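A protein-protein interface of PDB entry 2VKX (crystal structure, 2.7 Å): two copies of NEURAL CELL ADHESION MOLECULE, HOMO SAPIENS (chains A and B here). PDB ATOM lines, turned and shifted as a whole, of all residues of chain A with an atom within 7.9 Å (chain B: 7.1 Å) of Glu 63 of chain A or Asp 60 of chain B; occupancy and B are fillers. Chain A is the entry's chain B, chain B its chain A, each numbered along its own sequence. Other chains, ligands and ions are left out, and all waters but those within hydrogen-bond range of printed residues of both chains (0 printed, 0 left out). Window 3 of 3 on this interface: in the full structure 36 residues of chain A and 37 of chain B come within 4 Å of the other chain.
Glu 63 of chain A touches just these residues of chain B: Tyr 59 (3.8 Å), Asp 60 (3.2 Å) and Glu 63 (3.3 Å). Of chain A, only Glu 63 (3.2 Å) comes within 4 Å of Asp 60 of chain B. No residue of chain A comes within 4 Å of Ala 61 of chain B. Of the printed residues of chain B, Met 66 of chain A touches Lys 57 (3.7 Å). Of the printed residues of chain B, Lys 57 of chain A touches Glu 63 (3.8 Å) and Met 66 (3.3 Å). Printed residues of chain A within 4 Å of Met 66 of chain B: Lys 57 (3.3 Å). Lys 41 of chain A touches none of the printed residues of chain B. The nearest residue of chain B that does not touch Glu 63 of chain A is Trp 58 of chain B (4.3 Å). The nearest residue of chain A that does not touch Asp 60 of chain B is Asp 60 of chain A (5.7 Å).
Lys 57 of chain A touches Glu 63 of chain B, but with the chains exchanged Glu 63 of chain A does not touch Lys 57 of chain B (5.4 Å). Tyr 59 of chain A touches Glu 63 of chain B, and with the chains exchanged Glu 63 of chain A touches Tyr 59 of chain B. Asp 60 of chain A touches Glu 63 of chain B, and with the chains exchanged Glu 63 of chain A touches Asp 60 of chain B. Glu 63 of chain B touches its own counterpart, Glu 63 of chain A. Of the 10 pairs that touch across the chains among the printed residues, 7 have their exchanged pair printed and touching as well.
Hydrophobic or aromatic side chains of chain B that line the printed part of chain A: Tyr 59 and Met 66. Among the printed residues, 10 pairs touch across the chains. Among the printed residues, no Asp or Glu carboxylate lies within 4 Å of a Lys or Arg side-chain nitrogen of the other chain.
The backbone carbonyl oxygen of Tyr 42 of chain B lies within hydrogen-bond range of the backbone NH of Tyr 59 of chain B. The side-chain carboxylate (OD2) of Asp 60 of chain A is in hydrogen-bond range of the backbone NH (N) of Lys 62 of chain A. The side-chain amino group of Lys 41 of chain B lies within salt-bridge range of the side-chain carboxylate of Asp 60 of chain B (2.5 Å). The backbone NH of Glu 63 of chain B is in hydrogen-bond range of the side-chain carboxylate of Asp 60 of chain B (2.9 Å). The side-chain carboxylate of Asp 60 of chain B sits close to the backbone NH of Lys 62 of chain B, at 3.4 Å. The backbone NH (N) of Tyr 59 of chain A is in hydrogen-bond range of the backbone carbonyl oxygen (O) of Tyr 42 of chain A, at 3.0 Å.
NZ of Lys 57 of chain A touches CG of Glu 63 of chain B (3.8 Å). Lys 57 of chain A touches Met 66 of chain B (CE to CE, 3.3 Å). Tyr 59 of chain A touches Glu 63 of chain B (CA to OE2, 3.0 Å). Glu 63 of chain A touches Tyr 59 of chain B (OE1 to CD1, 3.8 Å). Lys 57 of chain B touches Met 66 of chain A (CE to CG, 3.7 Å). OE2 of Glu 67 of chain A touches OH of Tyr 59 of chain B, 3.6 Å away.
O of Trp 58 of chain A sits close to OE2 of Glu 63 of chain B. The side-chain carboxylate (OE2) of Glu 63 of chain A lies within hydrogen-bond range of the backbone NH (N) of Asp 60 of chain B (3.2 Å). OE2 of Glu 63 of chain B is in hydrogen-bond range of N of Asp 60 of chain A, 2.8 Å away. OE1 of Glu 63 of chain B sits close to OE1 of Glu 63 of chain A (3.3 Å).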
ATOM      1  N   LEU A  40      11.549 -11.983  18.313  1.00  0.00           N
ATOM      2  CA  LEU A  40      12.429 -13.140  18.143  1.00  0.00           C
ATOM      3  C   LEU A  40      12.258 -14.258  19.159  1.00  0.00           C
ATOM      4  O   LEU A  40      12.210 -15.437  18.802  1.00  0.00           O
ATOM      5  CB  LEU A  40      13.893 -12.689  18.185  1.00  0.00           C
ATOM      6  CG  LEU A  40      14.275 -11.458  17.358  1.00  0.00           C
ATOM      7  CD1 LEU A  40      15.723 -11.097  17.603  1.00  0.00           C
ATOM      8  CD2 LEU A  40      14.008 -11.726  15.886  1.00  0.00           C
ATOM      9  N   LYS A  41      12.192 -13.886  20.431  1.00  0.00           N
ATOM     10  CA  LYS A  41      12.074 -14.863  21.499  1.00  0.00           C
ATOM     11  C   LYS A  41      11.139 -14.380  22.594  1.00  0.00           C
ATOM     12  O   LYS A  41      10.726 -13.221  22.625  1.00  0.00           O
ATOM     13  CB  LYS A  41      13.450 -15.115  22.135  1.00  0.00           C
ATOM     14  CG  LYS A  41      14.570 -15.504  21.185  1.00  0.00           C
ATOM     15  CD  LYS A  41      14.365 -16.911  20.631  1.00  0.00           C
ATOM     16  CE  LYS A  41      15.480 -17.319  19.667  1.00  0.00           C
ATOM     17  NZ  LYS A  41      15.258 -18.696  19.152  1.00  0.00           N
ATOM     18  N   TYR A  42      10.822 -15.293  23.501  1.00  0.00           N
ATOM     19  CA  TYR A  42       9.978 -14.993  24.646  1.00  0.00           C
ATOM     20  C   TYR A  42      10.758 -15.435  25.862  1.00  0.00           C
ATOM     21  O   TYR A  42      11.408 -16.487  25.842  1.00  0.00           O
ATOM     22  CB  TYR A  42       8.655 -15.746  24.558  1.00  0.00           C
ATOM     23  CG  TYR A  42       7.704 -15.107  23.595  1.00  0.00           C
ATOM     24  CD1 TYR A  42       7.137 -13.867  23.880  1.00  0.00           C
ATOM     25  CD2 TYR A  42       7.412 -15.703  22.372  1.00  0.00           C
ATOM     26  CE1 TYR A  42       6.306 -13.231  22.970  1.00  0.00           C
ATOM     27  CE2 TYR A  42       6.584 -15.075  21.450  1.00  0.00           C
ATOM     28  CZ  TYR A  42       6.039 -13.837  21.755  1.00  0.00           C
ATOM     29  OH  TYR A  42       5.263 -13.181  20.832  1.00  0.00           O
ATOM     30  N   LYS A  57      14.184 -19.184  31.006  1.00  0.00           N
ATOM     31  CA  LYS A  57      14.455 -19.978  29.821  1.00  0.00           C
ATOM     32  C   LYS A  57      13.893 -19.215  28.624  1.00  0.00           C
ATOM     33  O   LYS A  57      12.844 -18.570  28.726  1.00  0.00           O
ATOM     34  CB  LYS A  57      13.770 -21.349  29.947  1.00  0.00           C
ATOM     35  CG  LYS A  57      14.005 -22.305  28.772  1.00  0.00           C
ATOM     36  CD  LYS A  57      15.471 -22.743  28.697  1.00  0.00           C
ATOM     37  CE  LYS A  57      15.731 -23.631  27.492  1.00  0.00           C
ATOM     38  NZ  LYS A  57      15.382 -22.917  26.232  1.00  0.00           N
ATOM     39  N   TRP A  58      14.601 -19.273  27.500  1.00  0.00           N
ATOM     40  CA  TRP A  58      14.149 -18.595  26.296  1.00  0.00           C
ATOM     41  C   TRP A  58      13.373 -19.562  25.424  1.00  0.00           C
ATOM     42  O   TRP A  58      13.662 -20.757  25.404  1.00  0.00           O
ATOM     43  CB  TRP A  58      15.330 -18.041  25.497  1.00  0.00           C
ATOM     44  CG  TRP A  58      16.028 -16.885  26.149  1.00  0.00           C
ATOM     45  CD1 TRP A  58      17.144 -16.935  26.936  1.00  0.00           C
ATOM     46  CD2 TRP A  58      15.641 -15.507  26.089  1.00  0.00           C
ATOM     47  NE1 TRP A  58      17.476 -15.669  27.373  1.00  0.00           N
ATOM     48  CE2 TRP A  58      16.570 -14.776  26.867  1.00  0.00           C
ATOM     49  CE3 TRP A  58      14.602 -14.820  25.456  1.00  0.00           C
ATOM     50  CZ2 TRP A  58      16.487 -13.392  27.028  1.00  0.00           C
ATOM     51  CZ3 TRP A  58      14.521 -13.444  25.615  1.00  0.00           C
ATOM     52  CH2 TRP A  58      15.460 -12.744  26.396  1.00  0.00           C
ATOM     53  N   TYR A  59      12.390 -19.037  24.701  1.00  0.00           N
ATOM     54  CA  TYR A  59      11.569 -19.849  23.815  1.00  0.00           C
ATOM     55  C   TYR A  59      11.481 -19.208  22.431  1.00  0.00           C
ATOM     56  O   TYR A  59      11.070 -18.056  22.290  1.00  0.00           O
ATOM     57  CB  TYR A  59      10.167 -20.002  24.411  1.00  0.00           C
ATOM     58  CG  TYR A  59      10.153 -20.775  25.708  1.00  0.00           C
ATOM     59  CD1 TYR A  59      10.105 -22.170  25.710  1.00  0.00           C
ATOM     60  CD2 TYR A  59      10.218 -20.114  26.936  1.00  0.00           C
ATOM     61  CE1 TYR A  59      10.116 -22.891  26.900  1.00  0.00           C
ATOM     62  CE2 TYR A  59      10.232 -20.823  28.133  1.00  0.00           C
ATOM     63  CZ  TYR A  59      10.176 -22.211  28.110  1.00  0.00           C
ATOM     64  OH  TYR A  59      10.138 -22.917  29.297  1.00  0.00           O
ATOM     65  N   ASP A  60      11.880 -19.948  21.409  1.00  0.00           N
ATOM     66  CA  ASP A  60      11.813 -19.415  20.063  1.00  0.00           C
ATOM     67  C   ASP A  60      10.402 -18.894  19.843  1.00  0.00           C
ATOM     68  O   ASP A  60       9.425 -19.589  20.115  1.00  0.00           O
ATOM     69  CB  ASP A  60      12.116 -20.494  19.029  1.00  0.00           C
ATOM     70  CG  ASP A  60      12.011 -19.970  17.621  1.00  0.00           C
ATOM     71  OD1 ASP A  60      12.857 -19.131  17.248  1.00  0.00           O
ATOM     72  OD2 ASP A  60      11.076 -20.374  16.894  1.00  0.00           O
ATOM     73  N   ALA A  61      10.292 -17.672  19.342  1.00  0.00           N
ATOM     74  CA  ALA A  61       8.988 -17.069  19.118  1.00  0.00           C
ATOM     75  C   ALA A  61       8.170 -17.786  18.056  1.00  0.00           C
ATOM     76  O   ALA A  61       6.973 -18.016  18.234  1.00  0.00           O
ATOM     77  CB  ALA A  61       9.153 -15.607  18.744  1.00  0.00           C
ATOM     78  N   LYS A  62       8.809 -18.145  16.952  1.00  0.00           N
ATOM     79  CA  LYS A  62       8.096 -18.808  15.870  1.00  0.00           C
ATOM     80  C   LYS A  62       7.477 -20.131  16.312  1.00  0.00           C
ATOM     81  O   LYS A  62       6.291 -20.371  16.082  1.00  0.00           O
ATOM     82  CB  LYS A  62       9.040 -19.036  14.689  1.00  0.00           C
ATOM     83  CG  LYS A  62       8.323 -19.210  13.352  1.00  0.00           C
ATOM     84  CD  LYS A  62       9.308 -19.170  12.186  1.00  0.00           C
ATOM     85  CE  LYS A  62      10.236 -17.946  12.253  1.00  0.00           C
ATOM     86  NZ  LYS A  62       9.507 -16.640  12.265  1.00  0.00           N
ATOM     87  N   GLU A  63       8.288 -20.976  16.949  1.00  0.00           N
ATOM     88  CA  GLU A  63       7.851 -22.281  17.440  1.00  0.00           C
ATOM     89  C   GLU A  63       6.727 -22.110  18.452  1.00  0.00           C
ATOM     90  O   GLU A  63       5.711 -22.802  18.386  1.00  0.00           O
ATOM     91  CB  GLU A  63       9.033 -23.010  18.075  1.00  0.00           C
ATOM     92  CG  GLU A  63       8.742 -24.388  18.625  1.00  0.00           C
ATOM     93  CD  GLU A  63      10.023 -25.195  18.853  1.00  0.00           C
ATOM     94  OE1 GLU A  63      10.122 -25.898  19.887  1.00  0.00           O
ATOM     95  OE2 GLU A  63      10.929 -25.131  17.984  1.00  0.00           O
ATOM     96  N   ALA A  64       6.908 -21.176  19.382  1.00  0.00           N
ATOM     97  CA  ALA A  64       5.889 -20.913  20.387  1.00  0.00           C
ATOM     98  C   ALA A  64       4.563 -20.537  19.723  1.00  0.00           C
ATOM     99  O   ALA A  64       3.505 -21.042  20.093  1.00  0.00           O
ATOM    100  CB  ALA A  64       6.351 -19.790  21.317  1.00  0.00           C
ATOM    101  N   SER A  65       4.633 -19.657  18.733  1.00  0.00           N
ATOM    102  CA  SER A  65       3.447 -19.195  18.026  1.00  0.00           C
ATOM    103  C   SER A  65       2.672 -20.294  17.312  1.00  0.00           C
ATOM    104  O   SER A  65       1.453 -20.208  17.161  1.00  0.00           O
ATOM    105  CB  SER A  65       3.844 -18.117  17.028  1.00  0.00           C
ATOM    106  OG  SER A  65       4.625 -17.121  17.670  1.00  0.00           O
ATOM    107  N   MET A  66       3.373 -21.329  16.872  1.00  0.00           N
ATOM    108  CA  MET A  66       2.714 -22.429  16.184  1.00  0.00           C
ATOM    109  C   MET A  66       2.220 -23.443  17.218  1.00  0.00           C
ATOM    110  O   MET A  66       1.223 -24.114  17.014  1.00  0.00           O
ATOM    111  CB  MET A  66       3.686 -23.091  15.201  1.00  0.00           C
ATOM    112  CG  MET A  66       3.003 -23.822  14.051  1.00  0.00           C
ATOM    113  SD  MET A  66       2.169 -22.706  12.878  1.00  0.00           S
ATOM    114  CE  MET A  66       2.265 -23.672  11.352  1.00  0.00           C
ATOM    115  N   GLU A  67       2.925 -23.536  18.336  1.00  0.00           N
ATOM    116  CA  GLU A  67       2.560 -24.448  19.404  1.00  0.00           C
ATOM    117  C   GLU A  67       1.357 -23.956  20.193  1.00  0.00           C
ATOM    118  O   GLU A  67       0.416 -24.713  20.452  1.00  0.00           O
ATOM    119  CB  GLU A  67       3.741 -24.642  20.351  1.00  0.00           C
ATOM    120  CG  GLU A  67       4.734 -25.680  19.870  1.00  0.00           C
ATOM    121  CD  GLU A  67       4.206 -27.105  20.007  1.00  0.00           C
ATOM    122  OE1 GLU A  67       4.047 -27.574  21.166  1.00  0.00           O
ATOM    123  OE2 GLU A  67       3.951 -27.745  18.957  1.00  0.00           O
ATOM    124  N   GLY A  68       1.389 -22.685  20.575  1.00  0.00           N
ATOM    125  CA  GLY A  68       0.292 -22.127  21.344  1.00  0.00           C
ATOM    126  C   GLY A  68       0.626 -22.079  22.820  1.00  0.00           C
ATOM    127  O   GLY A  68      -0.126 -21.533  23.622  1.00  0.00           O
ATOM    128  N   ILE A  69       1.774 -22.635  23.175  1.00  0.00           N
ATOM    129  CA  ILE A  69       2.196 -22.665  24.560  1.00  0.00           C
ATOM    130  C   ILE A  69       3.707 -22.755  24.682  1.00  0.00           C
ATOM    131  O   ILE A  69       4.421 -22.979  23.704  1.00  0.00           O
ATOM    132  CB  ILE A  69       1.623 -23.909  25.318  1.00  0.00           C
ATOM    133  CG1 ILE A  69       2.050 -25.189  24.603  1.00  0.00           C
ATOM    134  CG2 ILE A  69       0.111 -23.837  25.423  1.00  0.00           C
ATOM    135  CD1 ILE A  69       1.558 -26.446  25.268  1.00  0.00           C
ATOM    136  N   VAL A  70       4.170 -22.553  25.908  1.00  0.00           N
ATOM    137  CA  VAL A  70       5.569 -22.674  26.262  1.00  0.00           C
ATOM    138  C   VAL A  70       5.488 -23.480  27.547  1.00  0.00           C
ATOM    139  O   VAL A  70       4.654 -23.207  28.413  1.00  0.00           O
ATOM    140  CB  VAL A  70       6.238 -21.336  26.536  1.00  0.00           C
ATOM    141  CG1 VAL A  70       6.528 -20.651  25.228  1.00  0.00           C
ATOM    142  CG2 VAL A  70       5.351 -20.474  27.422  1.00  0.00           C
ATOM    143  N   PHE B  28      12.894 -37.938  25.259  1.00  0.00           N
ATOM    144  CA  PHE B  28      13.750 -38.773  24.421  1.00  0.00           C
ATOM    145  C   PHE B  28      15.244 -38.542  24.634  1.00  0.00           C
ATOM    146  O   PHE B  28      15.663 -37.567  25.263  1.00  0.00           O
ATOM    147  CB  PHE B  28      13.431 -38.510  22.945  1.00  0.00           C
ATOM    148  CG  PHE B  28      13.872 -37.153  22.482  1.00  0.00           C
ATOM    149  CD1 PHE B  28      15.034 -37.003  21.729  1.00  0.00           C
ATOM    150  CD2 PHE B  28      13.185 -36.009  22.891  1.00  0.00           C
ATOM    151  CE1 PHE B  28      15.515 -35.734  21.398  1.00  0.00           C
ATOM    152  CE2 PHE B  28      13.657 -34.735  22.566  1.00  0.00           C
ATOM    153  CZ  PHE B  28      14.826 -34.599  21.820  1.00  0.00           C
ATOM    154  N   ILE B  39      23.144 -32.061  15.235  1.00  0.00           N
ATOM    155  CA  ILE B  39      21.701 -32.184  15.041  1.00  0.00           C
ATOM    156  C   ILE B  39      21.044 -30.805  15.141  1.00  0.00           C
ATOM    157  O   ILE B  39      21.223 -30.083  16.123  1.00  0.00           O
ATOM    158  CB  ILE B  39      21.107 -33.140  16.087  1.00  0.00           C
ATOM    159  CG1 ILE B  39      21.834 -34.482  16.004  1.00  0.00           C
ATOM    160  CG2 ILE B  39      19.628 -33.347  15.834  1.00  0.00           C
ATOM    161  CD1 ILE B  39      21.559 -35.392  17.156  1.00  0.00           C
ATOM    162  N   LEU B  40      20.285 -30.450  14.111  1.00  0.00           N
ATOM    163  CA  LEU B  40      19.623 -29.154  14.042  1.00  0.00           C
ATOM    164  C   LEU B  40      18.176 -29.144  14.528  1.00  0.00           C
ATOM    165  O   LEU B  40      17.788 -28.287  15.327  1.00  0.00           O
ATOM    166  CB  LEU B  40      19.650 -28.642  12.603  1.00  0.00           C
ATOM    167  CG  LEU B  40      21.011 -28.593  11.912  1.00  0.00           C
ATOM    168  CD1 LEU B  40      20.792 -28.298  10.435  1.00  0.00           C
ATOM    169  CD2 LEU B  40      21.906 -27.549  12.568  1.00  0.00           C
ATOM    170  N   LYS B  41      17.379 -30.083  14.023  1.00  0.00           N
ATOM    171  CA  LYS B  41      15.972 -30.165  14.392  1.00  0.00           C
ATOM    172  C   LYS B  41      15.507 -31.593  14.651  1.00  0.00           C
ATOM    173  O   LYS B  41      16.219 -32.564  14.383  1.00  0.00           O
ATOM    174  CB  LYS B  41      15.105 -29.551  13.285  1.00  0.00           C
ATOM    175  CG  LYS B  41      15.547 -28.160  12.862  1.00  0.00           C
ATOM    176  CD  LYS B  41      15.580 -27.200  14.061  1.00  0.00           C
ATOM    177  CE  LYS B  41      16.252 -25.863  13.731  1.00  0.00           C
ATOM    178  NZ  LYS B  41      16.243 -24.937  14.900  1.00  0.00           N
ATOM    179  N   TYR B  42      14.301 -31.705  15.190  1.00  0.00           N
ATOM    180  CA  TYR B  42      13.703 -32.998  15.466  1.00  0.00           C
ATOM    181  C   TYR B  42      12.346 -32.985  14.799  1.00  0.00           C
ATOM    182  O   TYR B  42      11.589 -32.033  14.962  1.00  0.00           O
ATOM    183  CB  TYR B  42      13.558 -33.213  16.973  1.00  0.00           C
ATOM    184  CG  TYR B  42      14.852 -33.628  17.645  1.00  0.00           C
ATOM    185  CD1 TYR B  42      15.363 -34.919  17.479  1.00  0.00           C
ATOM    186  CD2 TYR B  42      15.589 -32.721  18.407  1.00  0.00           C
ATOM    187  CE1 TYR B  42      16.577 -35.291  18.055  1.00  0.00           C
ATOM    188  CE2 TYR B  42      16.800 -33.080  18.982  1.00  0.00           C
ATOM    189  CZ  TYR B  42      17.294 -34.367  18.807  1.00  0.00           C
ATOM    190  OH  TYR B  42      18.496 -34.732  19.393  1.00  0.00           O
ATOM    191  N   LYS B  57       5.737 -32.085  12.769  1.00  0.00           N
ATOM    192  CA  LYS B  57       6.107 -30.787  13.316  1.00  0.00           C
ATOM    193  C   LYS B  57       7.606 -30.804  13.589  1.00  0.00           C
ATOM    194  O   LYS B  57       8.144 -31.821  14.037  1.00  0.00           O
ATOM    195  CB  LYS B  57       5.366 -30.522  14.628  1.00  0.00           C
ATOM    196  CG  LYS B  57       5.534 -29.106  15.156  1.00  0.00           C
ATOM    197  CD  LYS B  57       4.817 -28.101  14.241  1.00  0.00           C
ATOM    198  CE  LYS B  57       5.324 -26.669  14.425  1.00  0.00           C
ATOM    199  NZ  LYS B  57       6.785 -26.533  14.111  1.00  0.00           N
ATOM    200  N   TRP B  58       8.279 -29.690  13.303  1.00  0.00           N
ATOM    201  CA  TRP B  58       9.715 -29.569  13.560  1.00  0.00           C
ATOM    202  C   TRP B  58       9.953 -28.919  14.928  1.00  0.00           C
ATOM    203  O   TRP B  58       9.201 -28.048  15.358  1.00  0.00           O
ATOM    204  CB  TRP B  58      10.412 -28.716  12.485  1.00  0.00           C
ATOM    205  CG  TRP B  58      10.468 -29.330  11.129  1.00  0.00           C
ATOM    206  CD1 TRP B  58       9.662 -29.044  10.068  1.00  0.00           C
ATOM    207  CD2 TRP B  58      11.354 -30.365  10.692  1.00  0.00           C
ATOM    208  NE1 TRP B  58       9.987 -29.838   8.994  1.00  0.00           N
ATOM    209  CE2 TRP B  58      11.023 -30.661   9.349  1.00  0.00           C
ATOM    210  CE3 TRP B  58      12.398 -31.076  11.303  1.00  0.00           C
ATOM    211  CZ2 TRP B  58      11.694 -31.638   8.608  1.00  0.00           C
ATOM    212  CZ3 TRP B  58      13.069 -32.050  10.565  1.00  0.00           C
ATOM    213  CH2 TRP B  58      12.713 -32.321   9.233  1.00  0.00           C
ATOM    214  N   TYR B  59      11.011 -29.353  15.600  1.00  0.00           N
ATOM    215  CA  TYR B  59      11.378 -28.827  16.911  1.00  0.00           C
ATOM    216  C   TYR B  59      12.864 -28.454  16.881  1.00  0.00           C
ATOM    217  O   TYR B  59      13.681 -29.208  16.351  1.00  0.00           O
ATOM    218  CB  TYR B  59      11.124 -29.896  17.990  1.00  0.00           C
ATOM    219  CG  TYR B  59       9.662 -30.202  18.238  1.00  0.00           C
ATOM    220  CD1 TYR B  59       8.913 -29.421  19.108  1.00  0.00           C
ATOM    221  CD2 TYR B  59       9.017 -31.247  17.568  1.00  0.00           C
ATOM    222  CE1 TYR B  59       7.557 -29.664  19.308  1.00  0.00           C
ATOM    223  CE2 TYR B  59       7.667 -31.501  17.759  1.00  0.00           C
ATOM    224  CZ  TYR B  59       6.938 -30.705  18.635  1.00  0.00           C
ATOM    225  OH  TYR B  59       5.598 -30.945  18.867  1.00  0.00           O
ATOM    226  N   ASP B  60      13.213 -27.291  17.422  1.00  0.00           N
ATOM    227  CA  ASP B  60      14.609 -26.870  17.449  1.00  0.00           C
ATOM    228  C   ASP B  60      15.391 -27.793  18.377  1.00  0.00           C
ATOM    229  O   ASP B  60      15.018 -27.986  19.532  1.00  0.00           O
ATOM    230  CB  ASP B  60      14.729 -25.421  17.935  1.00  0.00           C
ATOM    231  CG  ASP B  60      16.175 -25.004  18.191  1.00  0.00           C
ATOM    232  OD1 ASP B  60      17.007 -25.090  17.262  1.00  0.00           O
ATOM    233  OD2 ASP B  60      16.485 -24.586  19.328  1.00  0.00           O
ATOM    234  N   ALA B  61      16.481 -28.359  17.872  1.00  0.00           N
ATOM    235  CA  ALA B  61      17.301 -29.273  18.662  1.00  0.00           C
ATOM    236  C   ALA B  61      17.830 -28.654  19.954  1.00  0.00           C
ATOM    237  O   ALA B  61      17.808 -29.293  21.009  1.00  0.00           O
ATOM    238  CB  ALA B  61      18.464 -29.799  17.820  1.00  0.00           C
ATOM    239  N   LYS B  62      18.307 -27.418  19.879  1.00  0.00           N
ATOM    240  CA  LYS B  62      18.843 -26.767  21.067  1.00  0.00           C
ATOM    241  C   LYS B  62      17.796 -26.596  22.161  1.00  0.00           C
ATOM    242  O   LYS B  62      18.094 -26.820  23.337  1.00  0.00           O
ATOM    243  CB  LYS B  62      19.453 -25.413  20.706  1.00  0.00           C
ATOM    244  CG  LYS B  62      20.962 -25.408  20.710  1.00  0.00           C
ATOM    245  CD  LYS B  62      21.523 -24.210  19.937  1.00  0.00           C
ATOM    246  CE  LYS B  62      23.059 -24.276  19.814  1.00  0.00           C
ATOM    247  NZ  LYS B  62      23.543 -25.571  19.238  1.00  0.00           N
ATOM    248  N   GLU B  63      16.577 -26.205  21.787  1.00  0.00           N
ATOM    249  CA  GLU B  63      15.526 -26.020  22.782  1.00  0.00           C
ATOM    250  C   GLU B  63      15.045 -27.372  23.289  1.00  0.00           C
ATOM    251  O   GLU B  63      14.842 -27.558  24.491  1.00  0.00           O
ATOM    252  CB  GLU B  63      14.341 -25.244  22.204  1.00  0.00           C
ATOM    253  CG  GLU B  63      13.538 -24.501  23.275  1.00  0.00           C
ATOM    254  CD  GLU B  63      12.412 -23.642  22.701  1.00  0.00           C
ATOM    255  OE1 GLU B  63      11.334 -24.195  22.377  1.00  0.00           O
ATOM    256  OE2 GLU B  63      12.615 -22.409  22.571  1.00  0.00           O
ATOM    257  N   ALA B  64      14.872 -28.312  22.368  1.00  0.00           N
ATOM    258  CA  ALA B  64      14.416 -29.649  22.712  1.00  0.00           C
ATOM    259  C   ALA B  64      15.311 -30.304  23.757  1.00  0.00           C
ATOM    260  O   ALA B  64      14.830 -30.895  24.720  1.00  0.00           O
ATOM    261  CB  ALA B  64      14.361 -30.515  21.460  1.00  0.00           C
ATOM    262  N   SER B  65      16.617 -30.184  23.569  1.00  0.00           N
ATOM    263  CA  SER B  65      17.568 -30.783  24.488  1.00  0.00           C
ATOM    264  C   SER B  65      17.680 -30.060  25.819  1.00  0.00           C
ATOM    265  O   SER B  65      18.038 -30.671  26.817  1.00  0.00           O
ATOM    266  CB  SER B  65      18.939 -30.873  23.821  1.00  0.00           C
ATOM    267  OG  SER B  65      18.863 -31.679  22.654  1.00  0.00           O
ATOM    268  N   MET B  66      17.387 -28.764  25.842  1.00  0.00           N
ATOM    269  CA  MET B  66      17.455 -28.002  27.084  1.00  0.00           C
ATOM    270  C   MET B  66      16.184 -28.193  27.885  1.00  0.00           C
ATOM    271  O   MET B  66      16.039 -27.658  28.981  1.00  0.00           O
ATOM    272  CB  MET B  66      17.637 -26.519  26.806  1.00  0.00           C
ATOM    273  CG  MET B  66      19.051 -26.037  26.989  1.00  0.00           C
ATOM    274  SD  MET B  66      19.132 -24.248  26.814  1.00  0.00           S
ATOM    275  CE  MET B  66      18.896 -23.698  28.556  1.00  0.00           C
ATOM    276  N   ILE B  69      12.301 -32.605  26.641  1.00  0.00           N
ATOM    277  CA  ILE B  69      11.043 -32.982  26.033  1.00  0.00           C
ATOM    278  C   ILE B  69      10.645 -32.156  24.818  1.00  0.00           C
ATOM    279  O   ILE B  69      11.248 -31.128  24.506  1.00  0.00           O
ATOM    280  CB  ILE B  69       9.885 -32.868  27.046  1.00  0.00           C
ATOM    281  CG1 ILE B  69       9.898 -31.465  27.672  1.00  0.00           C
ATOM    282  CG2 ILE B  69       9.985 -33.979  28.089  1.00  0.00           C
ATOM    283  CD1 ILE B  69       8.643 -31.104  28.454  1.00  0.00           C
ATOM    284  N   VAL B  70       9.612 -32.640  24.139  1.00  0.00           N
ATOM    285  CA  VAL B  70       9.025 -31.979  22.991  1.00  0.00           C
ATOM    286  C   VAL B  70       7.546 -32.285  23.178  1.00  0.00           C
ATOM    287  O   VAL B  70       7.175 -33.446  23.383  1.00  0.00           O
ATOM    288  CB  VAL B  70       9.514 -32.566  21.652  1.00  0.00           C
ATOM    289  CG1 VAL B  70      10.986 -32.314  21.493  1.00  0.00           C
ATOM    290  CG2 VAL B  70       9.212 -34.048  21.586  1.00  0.00           C
